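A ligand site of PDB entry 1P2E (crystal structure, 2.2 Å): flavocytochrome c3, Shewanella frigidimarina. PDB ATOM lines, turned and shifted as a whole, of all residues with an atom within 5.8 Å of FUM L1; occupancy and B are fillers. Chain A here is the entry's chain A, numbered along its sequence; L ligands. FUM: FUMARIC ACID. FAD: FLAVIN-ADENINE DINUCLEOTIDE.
An oxygen (OXT) of FUM L1 lies close to a nitrogen (N3) of FAD L2 (3.3 Å).
The backbone NH (N) of Gly 170 sits at hydrogen-bond distance from the side-chain hydroxyl (OG1) of Thr 377 (3.2 Å). The side-chain carboxylate (OE1) of Glu 378 lies within salt-bridge range of the guanidinium group (NH2) of Arg 381. The backbone NH of His 504 is in hydrogen-bond range of the backbone carbonyl oxygen of Gln 363. N of Ala 379 is in hydrogen-bond range of OG1 of Thr 377 (2.9 Å). The guanidinium group (NH1) of Arg 402 sits at hydrogen-bond distance from the side-chain amide oxygen (OE1) of Gln 363, 2.7 Å away. The side-chain amide nitrogen (NE2) of Gln 363 is in hydrogen-bond range of the backbone carbonyl oxygen (O) of Arg 544 (2.8 Å). The guanidinium group (NE) of Arg 402 lies within salt-bridge range of the side-chain carboxylate (OE1) of Glu 378 (3.0 Å).
The side-chain sulfur (SD) of Met 375 sits close to an oxygen (O8) of FUM L1 (3.8 Å). Merely in contact with FUM L1: Ala 169 and Gly 546. Hydrophobic or aromatic side chains within 4 Å of FUM L1: Ala 169, His 365, Met 375 and His 504. 11 residues have an atom within 4 Å of FUM L1: Ala 169, Gly 170, His 365, Met 375, Thr 377, Glu 378, Arg 402, His 504, Arg 544, Gly 546 and Gly 547. The nearest printed residue that does not touch FUM L1 is Met 236 (4.04 Å).
A ring nitrogen (NE2) of His 365 sits at hydrogen-bond distance from an oxygen (O8) of FUM L1 (2.8 Å). An oxygen (O4) of FAD L2 is in hydrogen-bond range of the backbone NH (N) of Ala 169, at 3.2 Å. O2 of FAD L2 is in hydrogen-bond range of N of Ala 549, at 3.0 Å. An oxygen (O2) of FAD L2 is in hydrogen-bond range of the backbone NH (N) of Asn 548 (3.5 Å). N of Gly 170 sits at hydrogen-bond distance from O4 of FAD L2 (2.8 Å). N of Gly 170 is in hydrogen-bond range of O7 of FUM L1, at 2.9 Å. O2 of FAD L2 sits close to N of Gly 547, at 3.4 Å. NE2 of His 504 sits at hydrogen-bond distance from O of FUM L1, at 3.0 Å. OXT of FUM L1 is in salt-bridge range of NH1 of Arg 544, 2.6 Å away. N of Gly 547 sits at hydrogen-bond distance from OXT of FUM L1, at 2.6 Å. The side-chain hydroxyl of Thr 377 sits at hydrogen-bond distance from an oxygen (O7) of FUM L1 (2.7 Å). An oxygen (O) of FUM L1 lies within salt-bridge range of the guanidinium group of Arg 402, 2.7 Å away. The backbone NH (N) of Gly 171 sits at hydrogen-bond distance from an oxygen (O4) of FAD L2, 2.9 Å away. N of Glu 378 sits at hydrogen-bond distance from O8 of FUM L1, 2.8 Å away. O of Gly 171 sits at hydrogen-bond distance from N3 of FAD L2, 2.7 Å away.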
ATOM      1  N   ALA A 168     -30.824 -16.417 -18.228  1.00  0.00           N
ATOM      2  CA  ALA A 168     -30.029 -16.091 -17.049  1.00  0.00           C
ATOM      3  C   ALA A 168     -30.061 -17.134 -15.926  1.00  0.00           C
ATOM      4  O   ALA A 168     -31.102 -17.634 -15.529  1.00  0.00           O
ATOM      5  CB  ALA A 168     -30.425 -14.690 -16.589  1.00  0.00           C
ATOM      6  N   ALA A 169     -28.899 -17.553 -15.372  1.00  0.00           N
ATOM      7  CA  ALA A 169     -28.850 -18.546 -14.314  1.00  0.00           C
ATOM      8  C   ALA A 169     -28.459 -17.984 -12.954  1.00  0.00           C
ATOM      9  O   ALA A 169     -29.223 -17.846 -11.958  1.00  0.00           O
ATOM     10  CB  ALA A 169     -27.846 -19.647 -14.656  1.00  0.00           C
ATOM     11  N   GLY A 170     -27.219 -17.536 -12.890  1.00  0.00           N
ATOM     12  CA  GLY A 170     -26.588 -17.016 -11.689  1.00  0.00           C
ATOM     13  C   GLY A 170     -27.453 -16.178 -10.780  1.00  0.00           C
ATOM     14  O   GLY A 170     -27.351 -16.418  -9.556  1.00  0.00           O
ATOM     15  N   GLY A 171     -28.129 -15.140 -11.273  1.00  0.00           N
ATOM     16  CA  GLY A 171     -28.807 -14.354 -10.232  1.00  0.00           C
ATOM     17  C   GLY A 171     -28.874 -12.870 -10.590  1.00  0.00           C
ATOM     18  O   GLY A 171     -28.250 -12.458 -11.580  1.00  0.00           O
ATOM     19  N   MET A 236     -21.091 -14.361  -6.866  1.00  0.00           N
ATOM     20  CA  MET A 236     -20.463 -14.431  -8.170  1.00  0.00           C
ATOM     21  C   MET A 236     -19.212 -13.570  -8.094  1.00  0.00           C
ATOM     22  O   MET A 236     -19.154 -12.744  -7.167  1.00  0.00           O
ATOM     23  CB  MET A 236     -21.336 -14.080  -9.368  1.00  0.00           C
ATOM     24  CG  MET A 236     -22.319 -15.257  -9.620  1.00  0.00           C
ATOM     25  SD  MET A 236     -23.136 -15.129 -11.168  1.00  0.00           S
ATOM     26  CE  MET A 236     -24.513 -14.049 -10.759  1.00  0.00           C
ATOM     27  N   GLN A 363     -17.509  -8.512 -23.153  1.00  0.00           N
ATOM     28  CA  GLN A 363     -17.250  -9.536 -22.181  1.00  0.00           C
ATOM     29  C   GLN A 363     -17.408 -10.953 -22.763  1.00  0.00           C
ATOM     30  O   GLN A 363     -18.390 -11.297 -23.428  1.00  0.00           O
ATOM     31  CB  GLN A 363     -18.287  -9.393 -21.019  1.00  0.00           C
ATOM     32  CG  GLN A 363     -18.075 -10.477 -19.996  1.00  0.00           C
ATOM     33  CD  GLN A 363     -18.765 -10.172 -18.669  1.00  0.00           C
ATOM     34  OE1 GLN A 363     -19.843 -10.717 -18.411  1.00  0.00           O
ATOM     35  NE2 GLN A 363     -18.161  -9.339 -17.826  1.00  0.00           N
ATOM     36  N   HIS A 365     -17.683 -14.712 -21.534  1.00  0.00           N
ATOM     37  CA  HIS A 365     -17.918 -15.512 -20.340  1.00  0.00           C
ATOM     38  C   HIS A 365     -16.862 -16.627 -20.351  1.00  0.00           C
ATOM     39  O   HIS A 365     -16.630 -17.355 -21.334  1.00  0.00           O
ATOM     40  CB  HIS A 365     -19.303 -16.087 -20.338  1.00  0.00           C
ATOM     41  CG  HIS A 365     -19.732 -16.837 -19.116  1.00  0.00           C
ATOM     42  ND1 HIS A 365     -19.233 -18.011 -18.585  1.00  0.00           N
ATOM     43  CD2 HIS A 365     -20.719 -16.477 -18.270  1.00  0.00           C
ATOM     44  CE1 HIS A 365     -19.901 -18.346 -17.517  1.00  0.00           C
ATOM     45  NE2 HIS A 365     -20.831 -17.421 -17.287  1.00  0.00           N
ATOM     46  N   MET A 375     -23.537 -21.765 -21.815  1.00  0.00           N
ATOM     47  CA  MET A 375     -23.014 -21.211 -20.622  1.00  0.00           C
ATOM     48  C   MET A 375     -23.170 -22.141 -19.408  1.00  0.00           C
ATOM     49  O   MET A 375     -24.261 -22.642 -19.184  1.00  0.00           O
ATOM     50  CB  MET A 375     -23.860 -19.976 -20.232  1.00  0.00           C
ATOM     51  CG  MET A 375     -23.369 -19.234 -19.001  1.00  0.00           C
ATOM     52  SD  MET A 375     -24.405 -17.888 -18.498  1.00  0.00           S
ATOM     53  CE  MET A 375     -23.537 -16.485 -18.181  1.00  0.00           C
ATOM     54  N   VAL A 376     -22.110 -22.240 -18.606  1.00  0.00           N
ATOM     55  CA  VAL A 376     -22.240 -22.946 -17.332  1.00  0.00           C
ATOM     56  C   VAL A 376     -22.165 -21.802 -16.313  1.00  0.00           C
ATOM     57  O   VAL A 376     -21.180 -21.042 -16.263  1.00  0.00           O
ATOM     58  CB  VAL A 376     -21.173 -24.037 -17.124  1.00  0.00           C
ATOM     59  CG1 VAL A 376     -21.339 -24.761 -15.803  1.00  0.00           C
ATOM     60  CG2 VAL A 376     -21.210 -25.057 -18.283  1.00  0.00           C
ATOM     61  N   THR A 377     -23.225 -21.593 -15.552  1.00  0.00           N
ATOM     62  CA  THR A 377     -23.250 -20.458 -14.635  1.00  0.00           C
ATOM     63  C   THR A 377     -22.000 -20.430 -13.784  1.00  0.00           C
ATOM     64  O   THR A 377     -21.447 -21.369 -13.153  1.00  0.00           O
ATOM     65  CB  THR A 377     -24.525 -20.434 -13.799  1.00  0.00           C
ATOM     66  OG1 THR A 377     -24.529 -19.320 -12.910  1.00  0.00           O
ATOM     67  CG2 THR A 377     -24.784 -21.689 -13.004  1.00  0.00           C
ATOM     68  N   GLU A 378     -21.543 -19.215 -13.584  1.00  0.00           N
ATOM     69  CA  GLU A 378     -20.554 -18.828 -12.579  1.00  0.00           C
ATOM     70  C   GLU A 378     -21.115 -19.103 -11.202  1.00  0.00           C
ATOM     71  O   GLU A 378     -20.239 -19.268 -10.333  1.00  0.00           O
ATOM     72  CB  GLU A 378     -20.206 -17.349 -12.673  1.00  0.00           C
ATOM     73  CG  GLU A 378     -19.014 -16.814 -11.916  1.00  0.00           C
ATOM     74  CD  GLU A 378     -18.653 -15.486 -12.620  1.00  0.00           C
ATOM     75  OE1 GLU A 378     -18.301 -15.514 -13.832  1.00  0.00           O
ATOM     76  OE2 GLU A 378     -18.672 -14.540 -11.843  1.00  0.00           O
ATOM     77  N   ALA A 379     -22.422 -19.293 -10.938  1.00  0.00           N
ATOM     78  CA  ALA A 379     -22.867 -19.708  -9.635  1.00  0.00           C
ATOM     79  C   ALA A 379     -22.290 -21.112  -9.280  1.00  0.00           C
ATOM     80  O   ALA A 379     -22.191 -21.409  -8.097  1.00  0.00           O
ATOM     81  CB  ALA A 379     -24.366 -19.763  -9.394  1.00  0.00           C
ATOM     82  N   ARG A 381     -19.110 -21.851  -9.583  1.00  0.00           N
ATOM     83  CA  ARG A 381     -17.884 -21.601  -8.845  1.00  0.00           C
ATOM     84  C   ARG A 381     -18.199 -20.825  -7.565  1.00  0.00           C
ATOM     85  O   ARG A 381     -17.706 -21.271  -6.538  1.00  0.00           O
ATOM     86  CB  ARG A 381     -16.889 -20.849  -9.712  1.00  0.00           C
ATOM     87  CG  ARG A 381     -16.438 -21.592 -10.960  1.00  0.00           C
ATOM     88  CD  ARG A 381     -15.663 -20.613 -11.874  1.00  0.00           C
ATOM     89  NE  ARG A 381     -16.579 -20.067 -12.882  1.00  0.00           N
ATOM     90  CZ  ARG A 381     -16.656 -18.819 -13.368  1.00  0.00           C
ATOM     91  NH1 ARG A 381     -15.879 -17.839 -12.905  1.00  0.00           N
ATOM     92  NH2 ARG A 381     -17.487 -18.501 -14.351  1.00  0.00           N
ATOM     93  N   ARG A 402     -14.111 -11.725 -15.033  1.00  0.00           N
ATOM     94  CA  ARG A 402     -14.306 -12.560 -16.240  1.00  0.00           C
ATOM     95  C   ARG A 402     -13.164 -12.546 -17.223  1.00  0.00           C
ATOM     96  O   ARG A 402     -12.822 -13.549 -17.821  1.00  0.00           O
ATOM     97  CB  ARG A 402     -15.647 -12.148 -16.905  1.00  0.00           C
ATOM     98  CG  ARG A 402     -16.684 -12.718 -15.942  1.00  0.00           C
ATOM     99  CD  ARG A 402     -18.024 -12.651 -16.580  1.00  0.00           C
ATOM    100  NE  ARG A 402     -19.004 -13.360 -15.799  1.00  0.00           N
ATOM    101  CZ  ARG A 402     -20.319 -13.305 -15.804  1.00  0.00           C
ATOM    102  NH1 ARG A 402     -20.928 -12.435 -16.589  1.00  0.00           N
ATOM    103  NH2 ARG A 402     -20.916 -14.143 -14.964  1.00  0.00           N
ATOM    104  N   HIS A 504     -20.191 -13.110 -24.629  1.00  0.00           N
ATOM    105  CA  HIS A 504     -21.411 -13.136 -23.860  1.00  0.00           C
ATOM    106  C   HIS A 504     -22.237 -11.870 -23.701  1.00  0.00           C
ATOM    107  O   HIS A 504     -23.451 -11.937 -23.637  1.00  0.00           O
ATOM    108  CB  HIS A 504     -20.772 -13.494 -22.493  1.00  0.00           C
ATOM    109  CG  HIS A 504     -21.773 -13.688 -21.400  1.00  0.00           C
ATOM    110  ND1 HIS A 504     -22.766 -14.656 -21.613  1.00  0.00           N
ATOM    111  CD2 HIS A 504     -21.943 -13.147 -20.184  1.00  0.00           C
ATOM    112  CE1 HIS A 504     -23.548 -14.673 -20.555  1.00  0.00           C
ATOM    113  NE2 HIS A 504     -23.048 -13.781 -19.659  1.00  0.00           N
ATOM    114  N   ARG A 544     -18.542  -5.948 -16.806  1.00  0.00           N
ATOM    115  CA  ARG A 544     -19.748  -6.081 -15.962  1.00  0.00           C
ATOM    116  C   ARG A 544     -19.537  -7.197 -14.948  1.00  0.00           C
ATOM    117  O   ARG A 544     -18.958  -8.188 -15.391  1.00  0.00           O
ATOM    118  CB  ARG A 544     -20.951  -6.481 -16.829  1.00  0.00           C
ATOM    119  CG  ARG A 544     -22.263  -6.593 -16.057  1.00  0.00           C
ATOM    120  CD  ARG A 544     -23.423  -6.827 -16.974  1.00  0.00           C
ATOM    121  NE  ARG A 544     -23.344  -8.071 -17.763  1.00  0.00           N
ATOM    122  CZ  ARG A 544     -23.546  -9.291 -17.308  1.00  0.00           C
ATOM    123  NH1 ARG A 544     -23.786  -9.592 -16.024  1.00  0.00           N
ATOM    124  NH2 ARG A 544     -23.525 -10.320 -18.113  1.00  0.00           N
ATOM    125  N   LEU A 545     -20.110  -7.068 -13.760  1.00  0.00           N
ATOM    126  CA  LEU A 545     -20.021  -8.112 -12.764  1.00  0.00           C
ATOM    127  C   LEU A 545     -21.138  -9.124 -12.952  1.00  0.00           C
ATOM    128  O   LEU A 545     -22.279  -8.720 -13.196  1.00  0.00           O
ATOM    129  CB  LEU A 545     -20.064  -7.537 -11.341  1.00  0.00           C
ATOM    130  CG  LEU A 545     -19.096  -6.452 -10.899  1.00  0.00           C
ATOM    131  CD1 LEU A 545     -19.233  -6.183  -9.388  1.00  0.00           C
ATOM    132  CD2 LEU A 545     -17.682  -6.845 -11.199  1.00  0.00           C
ATOM    133  N   GLY A 546     -20.858 -10.412 -12.759  1.00  0.00           N
ATOM    134  CA  GLY A 546     -21.954 -11.400 -12.902  1.00  0.00           C
ATOM    135  C   GLY A 546     -23.098 -10.961 -12.026  1.00  0.00           C
ATOM    136  O   GLY A 546     -22.859 -10.587 -10.856  1.00  0.00           O
ATOM    137  N   GLY A 547     -24.358 -11.035 -12.554  1.00  0.00           N
ATOM    138  CA  GLY A 547     -25.519 -10.656 -11.758  1.00  0.00           C
ATOM    139  C   GLY A 547     -26.021  -9.216 -11.927  1.00  0.00           C
ATOM    140  O   GLY A 547     -27.136  -8.879 -11.519  1.00  0.00           O
ATOM    141  N   ASN A 548     -25.167  -8.354 -12.507  1.00  0.00           N
ATOM    142  CA  ASN A 548     -25.509  -6.949 -12.647  1.00  0.00           C
ATOM    143  C   ASN A 548     -26.407  -6.742 -13.890  1.00  0.00           C
ATOM    144  O   ASN A 548     -27.136  -5.756 -13.788  1.00  0.00           O
ATOM    145  CB  ASN A 548     -24.263  -6.111 -12.700  1.00  0.00           C
ATOM    146  CG  ASN A 548     -23.925  -5.432 -11.351  1.00  0.00           C
ATOM    147  OD1 ASN A 548     -24.602  -5.612 -10.335  1.00  0.00           O
ATOM    148  ND2 ASN A 548     -22.859  -4.622 -11.365  1.00  0.00           N
ATOM    149  N   ALA A 549     -26.456  -7.694 -14.828  1.00  0.00           N
ATOM    150  CA  ALA A 549     -27.322  -7.386 -16.009  1.00  0.00           C
ATOM    151  C   ALA A 549     -28.778  -7.610 -15.661  1.00  0.00           C
ATOM    152  O   ALA A 549     -29.554  -6.787 -16.078  1.00  0.00           O
ATOM    153  CB  ALA A 549     -26.899  -8.217 -17.239  1.00  0.00           C
HETATM  154  OXT FUM L   1     -24.307 -11.960 -14.963  1.00  0.00           O
HETATM  155  C   FUM L   1     -23.983 -12.919 -15.654  1.00  0.00           C
HETATM  156  O   FUM L   1     -23.571 -12.883 -16.879  1.00  0.00           O
HETATM  157  C4  FUM L   1     -24.189 -14.169 -14.944  1.00  0.00           C
HETATM  158  C5  FUM L   1     -23.791 -15.273 -15.518  1.00  0.00           C
HETATM  159  C6  FUM L   1     -23.758 -16.649 -15.025  1.00  0.00           C
HETATM  160  O7  FUM L   1     -24.832 -17.128 -14.455  1.00  0.00           O
HETATM  161  O8  FUM L   1     -22.680 -17.280 -15.203  1.00  0.00           O
HETATM  162  PA  FAD L   2     -32.825  -9.337 -23.978  1.00  0.00           P
HETATM  163  O1A FAD L   2     -31.701  -9.813 -24.851  1.00  0.00           O
HETATM  164  O2A FAD L   2     -33.281 -10.151 -22.845  1.00  0.00           O
HETATM  165  O5B FAD L   2     -34.104  -8.938 -24.819  1.00  0.00           O
HETATM  166  C5B FAD L   2     -33.917  -8.235 -26.057  1.00  0.00           C
HETATM  167  C4B FAD L   2     -35.054  -8.619 -26.993  1.00  0.00           C
HETATM  168  O4B FAD L   2     -35.297  -7.645 -27.988  1.00  0.00           O
HETATM  169  C3B FAD L   2     -34.856  -9.915 -27.723  1.00  0.00           C
HETATM  170  O3B FAD L   2     -35.944 -10.738 -27.372  1.00  0.00           O
HETATM  171  C2B FAD L   2     -34.609  -9.458 -29.145  1.00  0.00           C
HETATM  172  O2B FAD L   2     -34.980 -10.485 -30.076  1.00  0.00           O
HETATM  173  C1B FAD L   2     -35.664  -8.291 -29.195  1.00  0.00           C
HETATM  174  N9A FAD L   2     -35.265  -7.379 -30.285  1.00  0.00           N
HETATM  175  C8A FAD L   2     -33.989  -7.035 -30.644  1.00  0.00           C
HETATM  176  N7A FAD L   2     -33.948  -6.213 -31.635  1.00  0.00           N
HETATM  177  C5A FAD L   2     -35.304  -5.974 -31.985  1.00  0.00           C
HETATM  178  C6A FAD L   2     -35.996  -5.153 -32.846  1.00  0.00           C
HETATM  179  N6A FAD L   2     -35.444  -4.297 -33.773  1.00  0.00           N
HETATM  180  N1A FAD L   2     -37.339  -5.308 -32.847  1.00  0.00           N
HETATM  181  C2A FAD L   2     -38.108  -6.075 -32.089  1.00  0.00           C
HETATM  182  N3A FAD L   2     -37.408  -6.898 -31.181  1.00  0.00           N
HETATM  183  C4A FAD L   2     -36.074  -6.756 -31.209  1.00  0.00           C
HETATM  184  N1  FAD L   2     -27.117 -11.492 -16.250  1.00  0.00           N
HETATM  185  C2  FAD L   2     -27.212 -11.576 -14.885  1.00  0.00           C
HETATM  186  O2  FAD L   2     -27.213 -10.524 -14.286  1.00  0.00           O
HETATM  187  N3  FAD L   2     -27.389 -12.727 -14.143  1.00  0.00           N
HETATM  188  C4  FAD L   2     -27.403 -14.010 -14.702  1.00  0.00           C
HETATM  189  O4  FAD L   2     -27.465 -15.032 -14.113  1.00  0.00           O
HETATM  190  C4X FAD L   2     -27.138 -13.921 -16.184  1.00  0.00           C
HETATM  191  N5  FAD L   2     -26.898 -15.076 -16.747  1.00  0.00           N
HETATM  192  C5X FAD L   2     -26.834 -15.022 -18.099  1.00  0.00           C
HETATM  193  C6  FAD L   2     -26.807 -16.327 -18.785  1.00  0.00           C
HETATM  194  C7  FAD L   2     -26.837 -16.277 -20.215  1.00  0.00           C
HETATM  195  C7M FAD L   2     -26.797 -17.422 -21.156  1.00  0.00           C
HETATM  196  C8  FAD L   2     -26.991 -14.965 -20.723  1.00  0.00           C
HETATM  197  C8M FAD L   2     -27.104 -14.794 -22.210  1.00  0.00           C
HETATM  198  C9  FAD L   2     -26.901 -13.687 -20.116  1.00  0.00           C
HETATM  199  C9A FAD L   2     -26.868 -13.799 -18.725  1.00  0.00           C
HETATM  200  N10 FAD L   2     -26.822 -12.562 -18.120  1.00  0.00           N
HETATM  201  C10 FAD L   2     -27.004 -12.634 -16.792  1.00  0.00           C
HETATM  202  C1' FAD L   2     -26.982 -11.438 -19.095  1.00  0.00           C
HETATM  203  C2' FAD L   2     -28.358 -11.278 -19.582  1.00  0.00           C
HETATM  204  O2' FAD L   2     -29.411 -12.127 -19.086  1.00  0.00           O
HETATM  205  C3' FAD L   2     -28.741  -9.868 -20.094  1.00  0.00           C
HETATM  206  O3' FAD L   2     -27.581  -9.064 -20.410  1.00  0.00           O
HETATM  207  C4' FAD L   2     -29.864  -9.495 -21.027  1.00  0.00           C
HETATM  208  O4' FAD L   2     -30.909 -10.514 -20.977  1.00  0.00           O
HETATM  209  C5' FAD L   2     -30.260  -8.044 -21.034  1.00  0.00           C
HETATM  210  O5' FAD L   2     -31.665  -8.196 -21.130  1.00  0.00           O
HETATM  211  P   FAD L   2     -32.487  -7.142 -22.086  1.00  0.00           P
HETATM  212  O1P FAD L   2     -33.914  -7.075 -21.838  1.00  0.00           O
HETATM  213  O2P FAD L   2     -31.756  -5.873 -21.996  1.00  0.00           O
HETATM  214  O3P FAD L   2     -32.268  -7.898 -23.472  1.00  0.00           O
